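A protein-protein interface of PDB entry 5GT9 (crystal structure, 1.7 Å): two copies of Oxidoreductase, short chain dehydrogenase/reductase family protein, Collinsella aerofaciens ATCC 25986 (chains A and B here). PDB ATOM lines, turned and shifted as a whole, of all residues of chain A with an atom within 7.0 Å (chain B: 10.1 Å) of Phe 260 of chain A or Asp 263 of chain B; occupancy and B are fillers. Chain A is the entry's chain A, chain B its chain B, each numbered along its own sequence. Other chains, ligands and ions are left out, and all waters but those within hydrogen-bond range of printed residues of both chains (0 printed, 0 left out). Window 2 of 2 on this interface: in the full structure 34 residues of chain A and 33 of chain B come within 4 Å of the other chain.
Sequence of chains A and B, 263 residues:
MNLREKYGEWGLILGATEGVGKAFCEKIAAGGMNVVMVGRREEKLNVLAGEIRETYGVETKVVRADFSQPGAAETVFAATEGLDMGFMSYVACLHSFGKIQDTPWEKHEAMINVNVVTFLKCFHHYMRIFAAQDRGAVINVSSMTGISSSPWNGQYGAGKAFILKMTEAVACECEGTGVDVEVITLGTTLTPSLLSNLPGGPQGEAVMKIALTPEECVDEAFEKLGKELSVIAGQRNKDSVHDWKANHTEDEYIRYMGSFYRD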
ATOM      1  N   MET A 144      13.479   7.650 -26.693  1.00  0.00           N
ATOM      2  CA  MET A 144      12.757   6.411 -26.598  1.00  0.00           C
ATOM      3  C   MET A 144      11.983   6.107 -27.882  1.00  0.00           C
ATOM      4  O   MET A 144      11.768   4.969 -28.202  1.00  0.00           O
ATOM      5  CB  MET A 144      11.791   6.565 -25.450  1.00  0.00           C
ATOM      6  CG  MET A 144      11.380   5.352 -24.789  1.00  0.00           C
ATOM      7  SD  MET A 144      12.892   4.670 -24.199  1.00  0.00           S
ATOM      8  CE  MET A 144      12.838   5.222 -22.503  1.00  0.00           C
ATOM      9  N   THR A 145      11.491   7.165 -28.534  1.00  0.00           N
ATOM     10  CA  THR A 145      10.753   6.982 -29.790  1.00  0.00           C
ATOM     11  C   THR A 145      11.604   6.342 -30.906  1.00  0.00           C
ATOM     12  O   THR A 145      11.044   5.734 -31.823  1.00  0.00           O
ATOM     13  CB  THR A 145      10.140   8.290 -30.349  1.00  0.00           C
ATOM     14  OG1 THR A 145      11.175   9.287 -30.507  1.00  0.00           O
ATOM     15  CG2 THR A 145       9.008   8.767 -29.399  1.00  0.00           C
ATOM     16  N   PRO A 151       4.082   6.777 -34.119  1.00  0.00           N
ATOM     17  CA  PRO A 151       2.814   7.056 -34.793  1.00  0.00           C
ATOM     18  C   PRO A 151       2.289   8.489 -34.561  1.00  0.00           C
ATOM     19  O   PRO A 151       2.305   8.967 -33.403  1.00  0.00           O
ATOM     20  CB  PRO A 151       1.858   6.025 -34.184  1.00  0.00           C
ATOM     21  CG  PRO A 151       2.795   4.881 -33.772  1.00  0.00           C
ATOM     22  CD  PRO A 151       3.989   5.609 -33.216  1.00  0.00           C
ATOM     23  N   TRP A 152       1.849   9.114 -35.609  1.00  0.00           N
ATOM     24  CA  TRP A 152       1.364  10.487 -35.562  1.00  0.00           C
ATOM     25  C   TRP A 152       2.495  11.531 -35.423  1.00  0.00           C
ATOM     26  O   TRP A 152       2.238  12.685 -35.381  1.00  0.00           O
ATOM     27  CB  TRP A 152       0.259  10.639 -34.514  1.00  0.00           C
ATOM     28  CG  TRP A 152      -1.151  10.267 -35.034  1.00  0.00           C
ATOM     29  CD1 TRP A 152      -2.069  11.094 -35.588  1.00  0.00           C
ATOM     30  CD2 TRP A 152      -1.740   8.954 -35.053  1.00  0.00           C
ATOM     31  NE1 TRP A 152      -3.198  10.388 -35.958  1.00  0.00           N
ATOM     32  CE2 TRP A 152      -3.011   9.076 -35.625  1.00  0.00           C
ATOM     33  CE3 TRP A 152      -1.308   7.711 -34.660  1.00  0.00           C
ATOM     34  CZ2 TRP A 152      -3.829   7.986 -35.787  1.00  0.00           C
ATOM     35  CZ3 TRP A 152      -2.109   6.656 -34.816  1.00  0.00           C
ATOM     36  CH2 TRP A 152      -3.352   6.785 -35.363  1.00  0.00           C
ATOM     37  N   THR A 188      11.506  10.454 -20.555  1.00  0.00           N
ATOM     38  CA  THR A 188      10.966  11.726 -20.108  1.00  0.00           C
ATOM     39  C   THR A 188      12.034  12.520 -19.365  1.00  0.00           C
ATOM     40  O   THR A 188      12.636  12.003 -18.433  1.00  0.00           O
ATOM     41  CB  THR A 188       9.755  11.521 -19.185  1.00  0.00           C
ATOM     42  OG1 THR A 188       8.800  10.689 -19.854  1.00  0.00           O
ATOM     43  CG2 THR A 188       9.075  12.855 -18.824  1.00  0.00           C
ATOM     44  N   ARG A 255       1.570  -0.305 -31.560  1.00  0.00           N
ATOM     45  CA  ARG A 255       0.155  -0.059 -31.327  1.00  0.00           C
ATOM     46  C   ARG A 255      -0.092   0.632 -29.987  1.00  0.00           C
ATOM     47  O   ARG A 255      -0.983   1.488 -29.931  1.00  0.00           O
ATOM     48  CB  ARG A 255      -0.672  -1.334 -31.449  1.00  0.00           C
ATOM     49  CG  ARG A 255      -0.833  -1.801 -32.874  1.00  0.00           C
ATOM     50  CD  ARG A 255      -1.703  -3.027 -32.951  1.00  0.00           C
ATOM     51  NE  ARG A 255      -1.914  -3.411 -34.341  1.00  0.00           N
ATOM     52  CZ  ARG A 255      -1.668  -4.585 -34.892  1.00  0.00           C
ATOM     53  NH1 ARG A 255      -1.146  -5.564 -34.187  1.00  0.00           N
ATOM     54  NH2 ARG A 255      -1.947  -4.735 -36.174  1.00  0.00           N
ATOM     55  N   TYR A 256       0.699   0.333 -28.980  1.00  0.00           N
ATOM     56  CA  TYR A 256       0.671   1.121 -27.706  1.00  0.00           C
ATOM     57  C   TYR A 256       0.982   2.604 -27.990  1.00  0.00           C
ATOM     58  O   TYR A 256       0.216   3.511 -27.634  1.00  0.00           O
ATOM     59  CB  TYR A 256       1.606   0.515 -26.666  1.00  0.00           C
ATOM     60  CG  TYR A 256       1.786   1.464 -25.508  1.00  0.00           C
ATOM     61  CD1 TYR A 256       2.774   2.442 -25.540  1.00  0.00           C
ATOM     62  CD2 TYR A 256       0.888   1.469 -24.433  1.00  0.00           C
ATOM     63  CE1 TYR A 256       2.911   3.350 -24.514  1.00  0.00           C
ATOM     64  CE2 TYR A 256       1.036   2.383 -23.387  1.00  0.00           C
ATOM     65  CZ  TYR A 256       2.049   3.312 -23.445  1.00  0.00           C
ATOM     66  OH  TYR A 256       2.233   4.281 -22.484  1.00  0.00           O
ATOM     67  N   MET A 257       2.056   2.866 -28.741  1.00  0.00           N
ATOM     68  CA  MET A 257       2.388   4.271 -29.091  1.00  0.00           C
ATOM     69  C   MET A 257       1.298   5.007 -29.882  1.00  0.00           C
ATOM     70  O   MET A 257       1.178   6.223 -29.765  1.00  0.00           O
ATOM     71  CB  MET A 257       3.716   4.376 -29.805  1.00  0.00           C
ATOM     72  CG  MET A 257       4.875   3.836 -29.023  1.00  0.00           C
ATOM     73  SD  MET A 257       5.200   4.797 -27.544  1.00  0.00           S
ATOM     74  CE  MET A 257       5.428   6.414 -28.201  1.00  0.00           C
ATOM     75  N   GLY A 258       0.556   4.285 -30.747  1.00  0.00           N
ATOM     76  CA  GLY A 258      -0.476   4.820 -31.591  1.00  0.00           C
ATOM     77  C   GLY A 258      -1.838   4.908 -30.877  1.00  0.00           C
ATOM     78  O   GLY A 258      -2.725   5.562 -31.370  1.00  0.00           O
ATOM     79  N   SER A 259      -1.916   4.300 -29.725  1.00  0.00           N
ATOM     80  CA  SER A 259      -3.231   4.108 -29.016  1.00  0.00           C
ATOM     81  C   SER A 259      -3.711   5.383 -28.348  1.00  0.00           C
ATOM     82  O   SER A 259      -4.701   5.338 -27.605  1.00  0.00           O
ATOM     83  CB  SER A 259      -3.113   3.081 -27.962  1.00  0.00           C
ATOM     84  OG  SER A 259      -2.402   3.512 -26.828  1.00  0.00           O
ATOM     85  N   PHE A 260      -2.968   6.480 -28.549  1.00  0.00           N
ATOM     86  CA  PHE A 260      -3.276   7.782 -27.942  1.00  0.00           C
ATOM     87  C   PHE A 260      -3.967   8.654 -28.943  1.00  0.00           C
ATOM     88  O   PHE A 260      -4.640   9.620 -28.596  1.00  0.00           O
ATOM     89  CB  PHE A 260      -2.002   8.408 -27.367  1.00  0.00           C
ATOM     90  CG  PHE A 260      -1.480   7.662 -26.211  1.00  0.00           C
ATOM     91  CD1 PHE A 260      -2.095   7.760 -24.987  1.00  0.00           C
ATOM     92  CD2 PHE A 260      -0.424   6.793 -26.334  1.00  0.00           C
ATOM     93  CE1 PHE A 260      -1.670   7.033 -23.901  1.00  0.00           C
ATOM     94  CE2 PHE A 260       0.018   6.085 -25.264  1.00  0.00           C
ATOM     95  CZ  PHE A 260      -0.584   6.189 -24.032  1.00  0.00           C
ATOM     96  N   TYR A 261      -3.918   8.262 -30.194  1.00  0.00           N
ATOM     97  CA  TYR A 261      -4.399   9.116 -31.240  1.00  0.00           C
ATOM     98  C   TYR A 261      -5.451   8.303 -31.848  1.00  0.00           C
ATOM     99  O   TYR A 261      -5.630   7.142 -31.445  1.00  0.00           O
ATOM    100  CB  TYR A 261      -3.217   9.487 -32.147  1.00  0.00           C
ATOM    101  CG  TYR A 261      -2.014   9.916 -31.309  1.00  0.00           C
ATOM    102  CD1 TYR A 261      -1.950  11.188 -30.720  1.00  0.00           C
ATOM    103  CD2 TYR A 261      -0.962   9.052 -31.073  1.00  0.00           C
ATOM    104  CE1 TYR A 261      -0.872  11.559 -29.968  1.00  0.00           C
ATOM    105  CE2 TYR A 261       0.098   9.408 -30.290  1.00  0.00           C
ATOM    106  CZ  TYR A 261       0.165  10.692 -29.773  1.00  0.00           C
ATOM    107  OH  TYR A 261       1.209  11.064 -28.981  1.00  0.00           O
ATOM    108  N   ARG A 262      -6.222   8.854 -32.765  1.00  0.00           N
ATOM    109  CA  ARG A 262      -7.166   8.003 -33.493  1.00  0.00           C
ATOM    110  C   ARG A 262      -7.604   8.861 -34.642  1.00  0.00           C
ATOM    111  O   ARG A 262      -7.509   8.433 -35.779  1.00  0.00           O
ATOM    112  CB  ARG A 262      -8.405   7.451 -32.654  1.00  0.00           C
ATOM    113  CG  ARG A 262      -8.202   6.973 -31.156  1.00  0.00           C
ATOM    114  CD  ARG A 262      -7.626   5.550 -30.914  1.00  0.00           C
ATOM    115  NE  ARG A 262      -7.190   5.298 -29.531  1.00  0.00           N
ATOM    116  CZ  ARG A 262      -7.024   4.058 -28.953  1.00  0.00           C
ATOM    117  NH1 ARG A 262      -6.642   3.901 -27.694  1.00  0.00           N
ATOM    118  NH2 ARG A 262      -7.204   2.944 -29.625  1.00  0.00           N
ATOM    119  N   LYS B  99      -7.522  12.364 -13.412  1.00  0.00           N
ATOM    120  CA  LYS B  99      -8.386  12.727 -14.518  1.00  0.00           C
ATOM    121  C   LYS B  99      -9.671  13.340 -14.007  1.00  0.00           C
ATOM    122  O   LYS B  99     -10.052  13.090 -12.876  1.00  0.00           O
ATOM    123  CB  LYS B  99      -8.697  11.548 -15.450  1.00  0.00           C
ATOM    124  CG  LYS B  99      -7.512  10.963 -16.188  1.00  0.00           C
ATOM    125  CD  LYS B  99      -8.035   9.946 -17.236  1.00  0.00           C
ATOM    126  CE  LYS B  99      -6.915   9.467 -18.192  1.00  0.00           C
ATOM    127  NZ  LYS B  99      -7.522   8.709 -19.316  1.00  0.00           N
ATOM    128  N   TRP B 152      -4.007  15.497 -16.110  1.00  0.00           N
ATOM    129  CA  TRP B 152      -4.085  14.744 -14.868  1.00  0.00           C
ATOM    130  C   TRP B 152      -4.171  15.563 -13.558  1.00  0.00           C
ATOM    131  O   TRP B 152      -4.152  15.035 -12.495  1.00  0.00           O
ATOM    132  CB  TRP B 152      -3.007  13.638 -14.833  1.00  0.00           C
ATOM    133  CG  TRP B 152      -3.312  12.428 -15.637  1.00  0.00           C
ATOM    134  CD1 TRP B 152      -3.793  11.251 -15.186  1.00  0.00           C
ATOM    135  CD2 TRP B 152      -3.174  12.278 -17.046  1.00  0.00           C
ATOM    136  NE1 TRP B 152      -3.960  10.375 -16.204  1.00  0.00           N
ATOM    137  CE2 TRP B 152      -3.564  10.973 -17.362  1.00  0.00           C
ATOM    138  CE3 TRP B 152      -2.683  13.079 -18.066  1.00  0.00           C
ATOM    139  CZ2 TRP B 152      -3.532  10.501 -18.650  1.00  0.00           C
ATOM    140  CZ3 TRP B 152      -2.658  12.610 -19.304  1.00  0.00           C
ATOM    141  CH2 TRP B 152      -3.089  11.320 -19.606  1.00  0.00           C
ATOM    142  N   ASP B 251      -1.069  22.484 -29.078  1.00  0.00           N
ATOM    143  CA  ASP B 251      -1.189  21.015 -28.827  1.00  0.00           C
ATOM    144  C   ASP B 251       0.158  20.394 -28.459  1.00  0.00           C
ATOM    145  O   ASP B 251       0.188  19.500 -27.659  1.00  0.00           O
ATOM    146  CB  ASP B 251      -1.721  20.278 -30.038  1.00  0.00           C
ATOM    147  CG  ASP B 251      -3.192  20.408 -30.247  1.00  0.00           C
ATOM    148  OD1 ASP B 251      -3.837  21.132 -29.527  1.00  0.00           O
ATOM    149  OD2 ASP B 251      -3.743  19.736 -31.170  1.00  0.00           O
ATOM    150  N   GLU B 252       1.256  20.897 -29.003  1.00  0.00           N
ATOM    151  CA  GLU B 252       2.566  20.298 -28.682  1.00  0.00           C
ATOM    152  C   GLU B 252       2.863  20.496 -27.172  1.00  0.00           C
ATOM    153  O   GLU B 252       3.362  19.591 -26.498  1.00  0.00           O
ATOM    154  CB  GLU B 252       3.689  20.920 -29.526  1.00  0.00           C
ATOM    155  CG  GLU B 252       3.732  20.395 -30.954  1.00  0.00           C
ATOM    156  CD  GLU B 252       4.786  21.059 -31.853  1.00  0.00           C
ATOM    157  OE1 GLU B 252       5.373  20.306 -32.696  1.00  0.00           O
ATOM    158  OE2 GLU B 252       4.990  22.299 -31.789  1.00  0.00           O
ATOM    159  N   ILE B 254       0.565  21.085 -24.832  1.00  0.00           N
ATOM    160  CA  ILE B 254      -0.392  20.291 -24.031  1.00  0.00           C
ATOM    161  C   ILE B 254       0.032  18.777 -23.929  1.00  0.00           C
ATOM    162  O   ILE B 254       0.080  18.176 -22.872  1.00  0.00           O
ATOM    163  CB  ILE B 254      -1.837  20.421 -24.587  1.00  0.00           C
ATOM    164  CG1 ILE B 254      -2.338  21.886 -24.545  1.00  0.00           C
ATOM    165  CG2 ILE B 254      -2.765  19.468 -23.884  1.00  0.00           C
ATOM    166  CD1 ILE B 254      -3.469  22.146 -25.514  1.00  0.00           C
ATOM    167  N   ARG B 255       0.398  18.212 -25.059  1.00  0.00           N
ATOM    168  CA  ARG B 255       0.813  16.776 -25.089  1.00  0.00           C
ATOM    169  C   ARG B 255       2.088  16.590 -24.284  1.00  0.00           C
ATOM    170  O   ARG B 255       2.202  15.610 -23.481  1.00  0.00           O
ATOM    171  CB  ARG B 255       0.940  16.299 -26.536  1.00  0.00           C
ATOM    172  CG  ARG B 255      -0.359  16.084 -27.211  1.00  0.00           C
ATOM    173  CD  ARG B 255      -0.244  15.388 -28.558  1.00  0.00           C
ATOM    174  NE  ARG B 255      -1.556  15.192 -29.186  1.00  0.00           N
ATOM    175  CZ  ARG B 255      -1.999  15.839 -30.282  1.00  0.00           C
ATOM    176  NH1 ARG B 255      -1.248  16.733 -30.933  1.00  0.00           N
ATOM    177  NH2 ARG B 255      -3.212  15.573 -30.747  1.00  0.00           N
ATOM    178  N   TYR B 256       3.028  17.527 -24.387  1.00  0.00           N
ATOM    179  CA  TYR B 256       4.249  17.495 -23.579  1.00  0.00           C
ATOM    180  C   TYR B 256       3.969  17.520 -22.082  1.00  0.00           C
ATOM    181  O   TYR B 256       4.586  16.784 -21.302  1.00  0.00           O
ATOM    182  CB  TYR B 256       5.227  18.586 -23.979  1.00  0.00           C
ATOM    183  CG  TYR B 256       6.615  18.449 -23.411  1.00  0.00           C
ATOM    184  CD1 TYR B 256       7.500  17.513 -23.940  1.00  0.00           C
ATOM    185  CD2 TYR B 256       7.050  19.237 -22.340  1.00  0.00           C
ATOM    186  CE1 TYR B 256       8.792  17.371 -23.448  1.00  0.00           C
ATOM    187  CE2 TYR B 256       8.340  19.065 -21.817  1.00  0.00           C
ATOM    188  CZ  TYR B 256       9.206  18.145 -22.377  1.00  0.00           C
ATOM    189  OH  TYR B 256      10.521  17.961 -21.843  1.00  0.00           O
ATOM    190  N   MET B 257       2.928  18.291 -21.673  1.00  0.00           N
ATOM    191  CA  MET B 257       2.587  18.375 -20.252  1.00  0.00           C
ATOM    192  C   MET B 257       2.003  17.090 -19.760  1.00  0.00           C
ATOM    193  O   MET B 257       1.905  16.890 -18.581  1.00  0.00           O
ATOM    194  CB  MET B 257       1.622  19.516 -19.947  1.00  0.00           C
ATOM    195  CG  MET B 257       2.199  20.909 -20.143  1.00  0.00           C
ATOM    196  SD  MET B 257       3.715  21.200 -19.208  1.00  0.00           S
ATOM    197  CE  MET B 257       3.190  20.772 -17.581  1.00  0.00           C
ATOM    198  N   GLY B 258       1.539  16.237 -20.668  1.00  0.00           N
ATOM    199  CA  GLY B 258       0.971  14.939 -20.272  1.00  0.00           C
ATOM    200  C   GLY B 258       2.038  13.856 -20.238  1.00  0.00           C
ATOM    201  O   GLY B 258       1.696  12.704 -20.028  1.00  0.00           O
ATOM    202  N   SER B 259       3.310  14.192 -20.483  1.00  0.00           N
ATOM    203  CA  SER B 259       4.376  13.187 -20.644  1.00  0.00           C
ATOM    204  C   SER B 259       4.489  12.127 -19.555  1.00  0.00           C
ATOM    205  O   SER B 259       5.023  11.024 -19.825  1.00  0.00           O
ATOM    206  CB  SER B 259       5.763  13.890 -20.669  1.00  0.00           C
ATOM    207  OG  SER B 259       5.906  14.568 -21.872  1.00  0.00           O
ATOM    208  N   PHE B 260       4.188  12.463 -18.312  1.00  0.00           N
ATOM    209  CA  PHE B 260       4.346  11.520 -17.226  1.00  0.00           C
ATOM    210  C   PHE B 260       3.342  10.384 -17.306  1.00  0.00           C
ATOM    211  O   PHE B 260       3.612   9.297 -16.751  1.00  0.00           O
ATOM    212  CB  PHE B 260       4.120  12.184 -15.875  1.00  0.00           C
ATOM    213  CG  PHE B 260       5.062  13.303 -15.558  1.00  0.00           C
ATOM    214  CD1 PHE B 260       6.382  13.229 -15.960  1.00  0.00           C
ATOM    215  CD2 PHE B 260       4.657  14.400 -14.812  1.00  0.00           C
ATOM    216  CE1 PHE B 260       7.261  14.231 -15.636  1.00  0.00           C
ATOM    217  CE2 PHE B 260       5.575  15.408 -14.462  1.00  0.00           C
ATOM    218  CZ  PHE B 260       6.854  15.316 -14.917  1.00  0.00           C
ATOM    219  N   TYR B 261       2.214  10.600 -18.014  1.00  0.00           N
ATOM    220  CA  TYR B 261       1.042   9.738 -17.899  1.00  0.00           C
ATOM    221  C   TYR B 261       0.629   9.102 -19.198  1.00  0.00           C
ATOM    222  O   TYR B 261      -0.266   8.250 -19.249  1.00  0.00           O
ATOM    223  CB  TYR B 261      -0.152  10.563 -17.312  1.00  0.00           C
ATOM    224  CG  TYR B 261       0.244  11.451 -16.155  1.00  0.00           C
ATOM    225  CD1 TYR B 261       0.543  10.913 -14.963  1.00  0.00           C
ATOM    226  CD2 TYR B 261       0.382  12.825 -16.316  1.00  0.00           C
ATOM    227  CE1 TYR B 261       0.954  11.697 -13.890  1.00  0.00           C
ATOM    228  CE2 TYR B 261       0.788  13.628 -15.264  1.00  0.00           C
ATOM    229  CZ  TYR B 261       1.052  13.049 -14.044  1.00  0.00           C
ATOM    230  OH  TYR B 261       1.463  13.832 -12.976  1.00  0.00           O
ATOM    231  N   ARG B 262       1.220   9.548 -20.289  1.00  0.00           N
ATOM    232  CA  ARG B 262       0.896   9.001 -21.594  1.00  0.00           C
ATOM    233  C   ARG B 262       2.095   9.203 -22.517  1.00  0.00           C
ATOM    234  O   ARG B 262       3.111   9.806 -22.131  1.00  0.00           O
ATOM    235  CB  ARG B 262      -0.341   9.686 -22.158  1.00  0.00           C
ATOM    236  CG  ARG B 262      -0.206  11.175 -22.101  1.00  0.00           C
ATOM    237  CD  ARG B 262      -1.034  11.821 -23.112  1.00  0.00           C
ATOM    238  NE  ARG B 262      -0.591  11.538 -24.480  1.00  0.00           N
ATOM    239  CZ  ARG B 262      -1.226  12.053 -25.513  1.00  0.00           C
ATOM    240  NH1 ARG B 262      -0.863  11.750 -26.751  1.00  0.00           N
ATOM    241  NH2 ARG B 262      -2.246  12.899 -25.257  1.00  0.00           N
ATOM    242  N   ASP B 263       1.929   8.765 -23.751  1.00  0.00           N
ATOM    243  CA  ASP B 263       2.973   8.832 -24.760  1.00  0.00           C
ATOM    244  C   ASP B 263       2.393   9.358 -26.052  1.00  0.00           C
ATOM    245  O   ASP B 263       1.243   9.794 -26.038  1.00  0.00           O
ATOM    246  CB  ASP B 263       3.577   7.453 -24.917  1.00  0.00           C
ATOM    247  CG  ASP B 263       4.407   7.091 -23.730  1.00  0.00           C
ATOM    248  OD1 ASP B 263       5.508   7.639 -23.627  1.00  0.00           O
ATOM    249  OD2 ASP B 263       3.974   6.319 -22.888  1.00  0.00           O
ATOM    250  OXT ASP B 263       3.087   9.384 -27.069  1.00  0.00           O
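The side-chain hydroxyl (OH) of Tyr 256 of chain A sits at hydrogen-bond distance from the side-chain carboxylate (OD2) of Asp 263 of chain B, at 2.7 Å. NH1 of Arg 262 of chain B lies within hydrogen-bond range of OH of Tyr 261 of chain A, at 3.1 Å. OXT of Asp 263 of chain B is in hydrogen-bond range of OH of Tyr 261 of chain A, 3.2 Å away.
The side-chain hydroxyl (OG) of Ser 259 of chain A is in hydrogen-bond range of the backbone carbonyl oxygen (O) of Tyr 256 of chain A (2.7 Å). NH1 of Arg 255 of chain B is in salt-bridge range of OD2 of Asp 251 of chain B (3.9 Å). The side-chain hydroxyl (OG) of Ser 259 of chain B lies within hydrogen-bond range of the backbone carbonyl oxygen (O) of Tyr 256 of chain B (2.6 Å).
Among the printed residues, pairs that only touch across the chains: Phe 260 of chain A with Arg 262 of chain B (3.4 Å), Phe 260 of chain A with Asp 263 of chain B (3.4 Å), Tyr 261 of chain A with Arg 255 of chain B (3.8 Å), Thr 188 of chain A with Ser 259 of chain B (3.8 Å), Met 257 of chain A with Asp 263 of chain B (3.9 Å) and Thr 188 of chain A with Phe 260 of chain B (3.9 Å).
Phe 260 of chain A touches just these residues of chain B: Arg 262 (3.4 Å) and Asp 263 (3.4 Å). Asp 263 of chain B touches four residues of chain A. Of the printed residues of chain B, Met 257 of chain A touches Asp 263. No residue of chain B comes within 4 Å of Gly 258 of chain A. No residue of chain B comes within 4 Å of Ser 259 of chain A. Tyr 261 of chain A touches just these residues of chain B: Arg 255, Arg 262 and Asp 263. Of the printed residues of chain B, Thr 188 of chain A touches Ser 259 (3.8 Å) and Phe 260 (3.9 Å). Of the printed residues of chain A, Phe 260 of chain B touches Thr 188. Of the printed residues of chain A, Ser 259 of chain B touches Thr 188 (3.8 Å). Thr 145 of chain A touches none of the printed residues of chain B. The nearest printed residue of chain A that does not touch Ser 259 of chain B is Tyr 256 of chain A (7.8 Å).
Hydrophobic or aromatic side chains of chain B within 4 Å of the printed part of chain A: Phe 260. Along chain B the printed residues that touch a printed residue of chain A span positions 255 to 263. Of the 13 printed residues of chain A, 5 touch a printed residue of chain B. Printed residues of chain A that touch a printed residue of chain B: Thr 188, Tyr 256, Met 257, Phe 260 and Tyr 261. Along chain A the printed residues that touch a printed residue of chain B span positions 188 to 261. Among the printed residues, 9 pairs touch across the chains. Among the printed residues, no Asp or Glu carboxylate lies within 4 Å of a Lys or Arg side-chain nitrogen of the other chain.
Phe 260 of chain A touches Arg 262 of chain B, but with the chains exchanged Arg 262 of chain A does not touch Phe 260 of chain B (15.8 Å). Tyr 261 of chain A touches Arg 255 of chain B, but with the chains exchanged Arg 255 of chain A does not touch Tyr 261 of chain B (12.7 Å). Tyr 261 of chain A touches Arg 262 of chain B, but with the chains exchanged Arg 262 of chain A does not touch Tyr 261 of chain B (11.4 Å). Of the 9 pairs that touch across the chains among the printed residues, none has its exchanged pair printed and touching as well.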
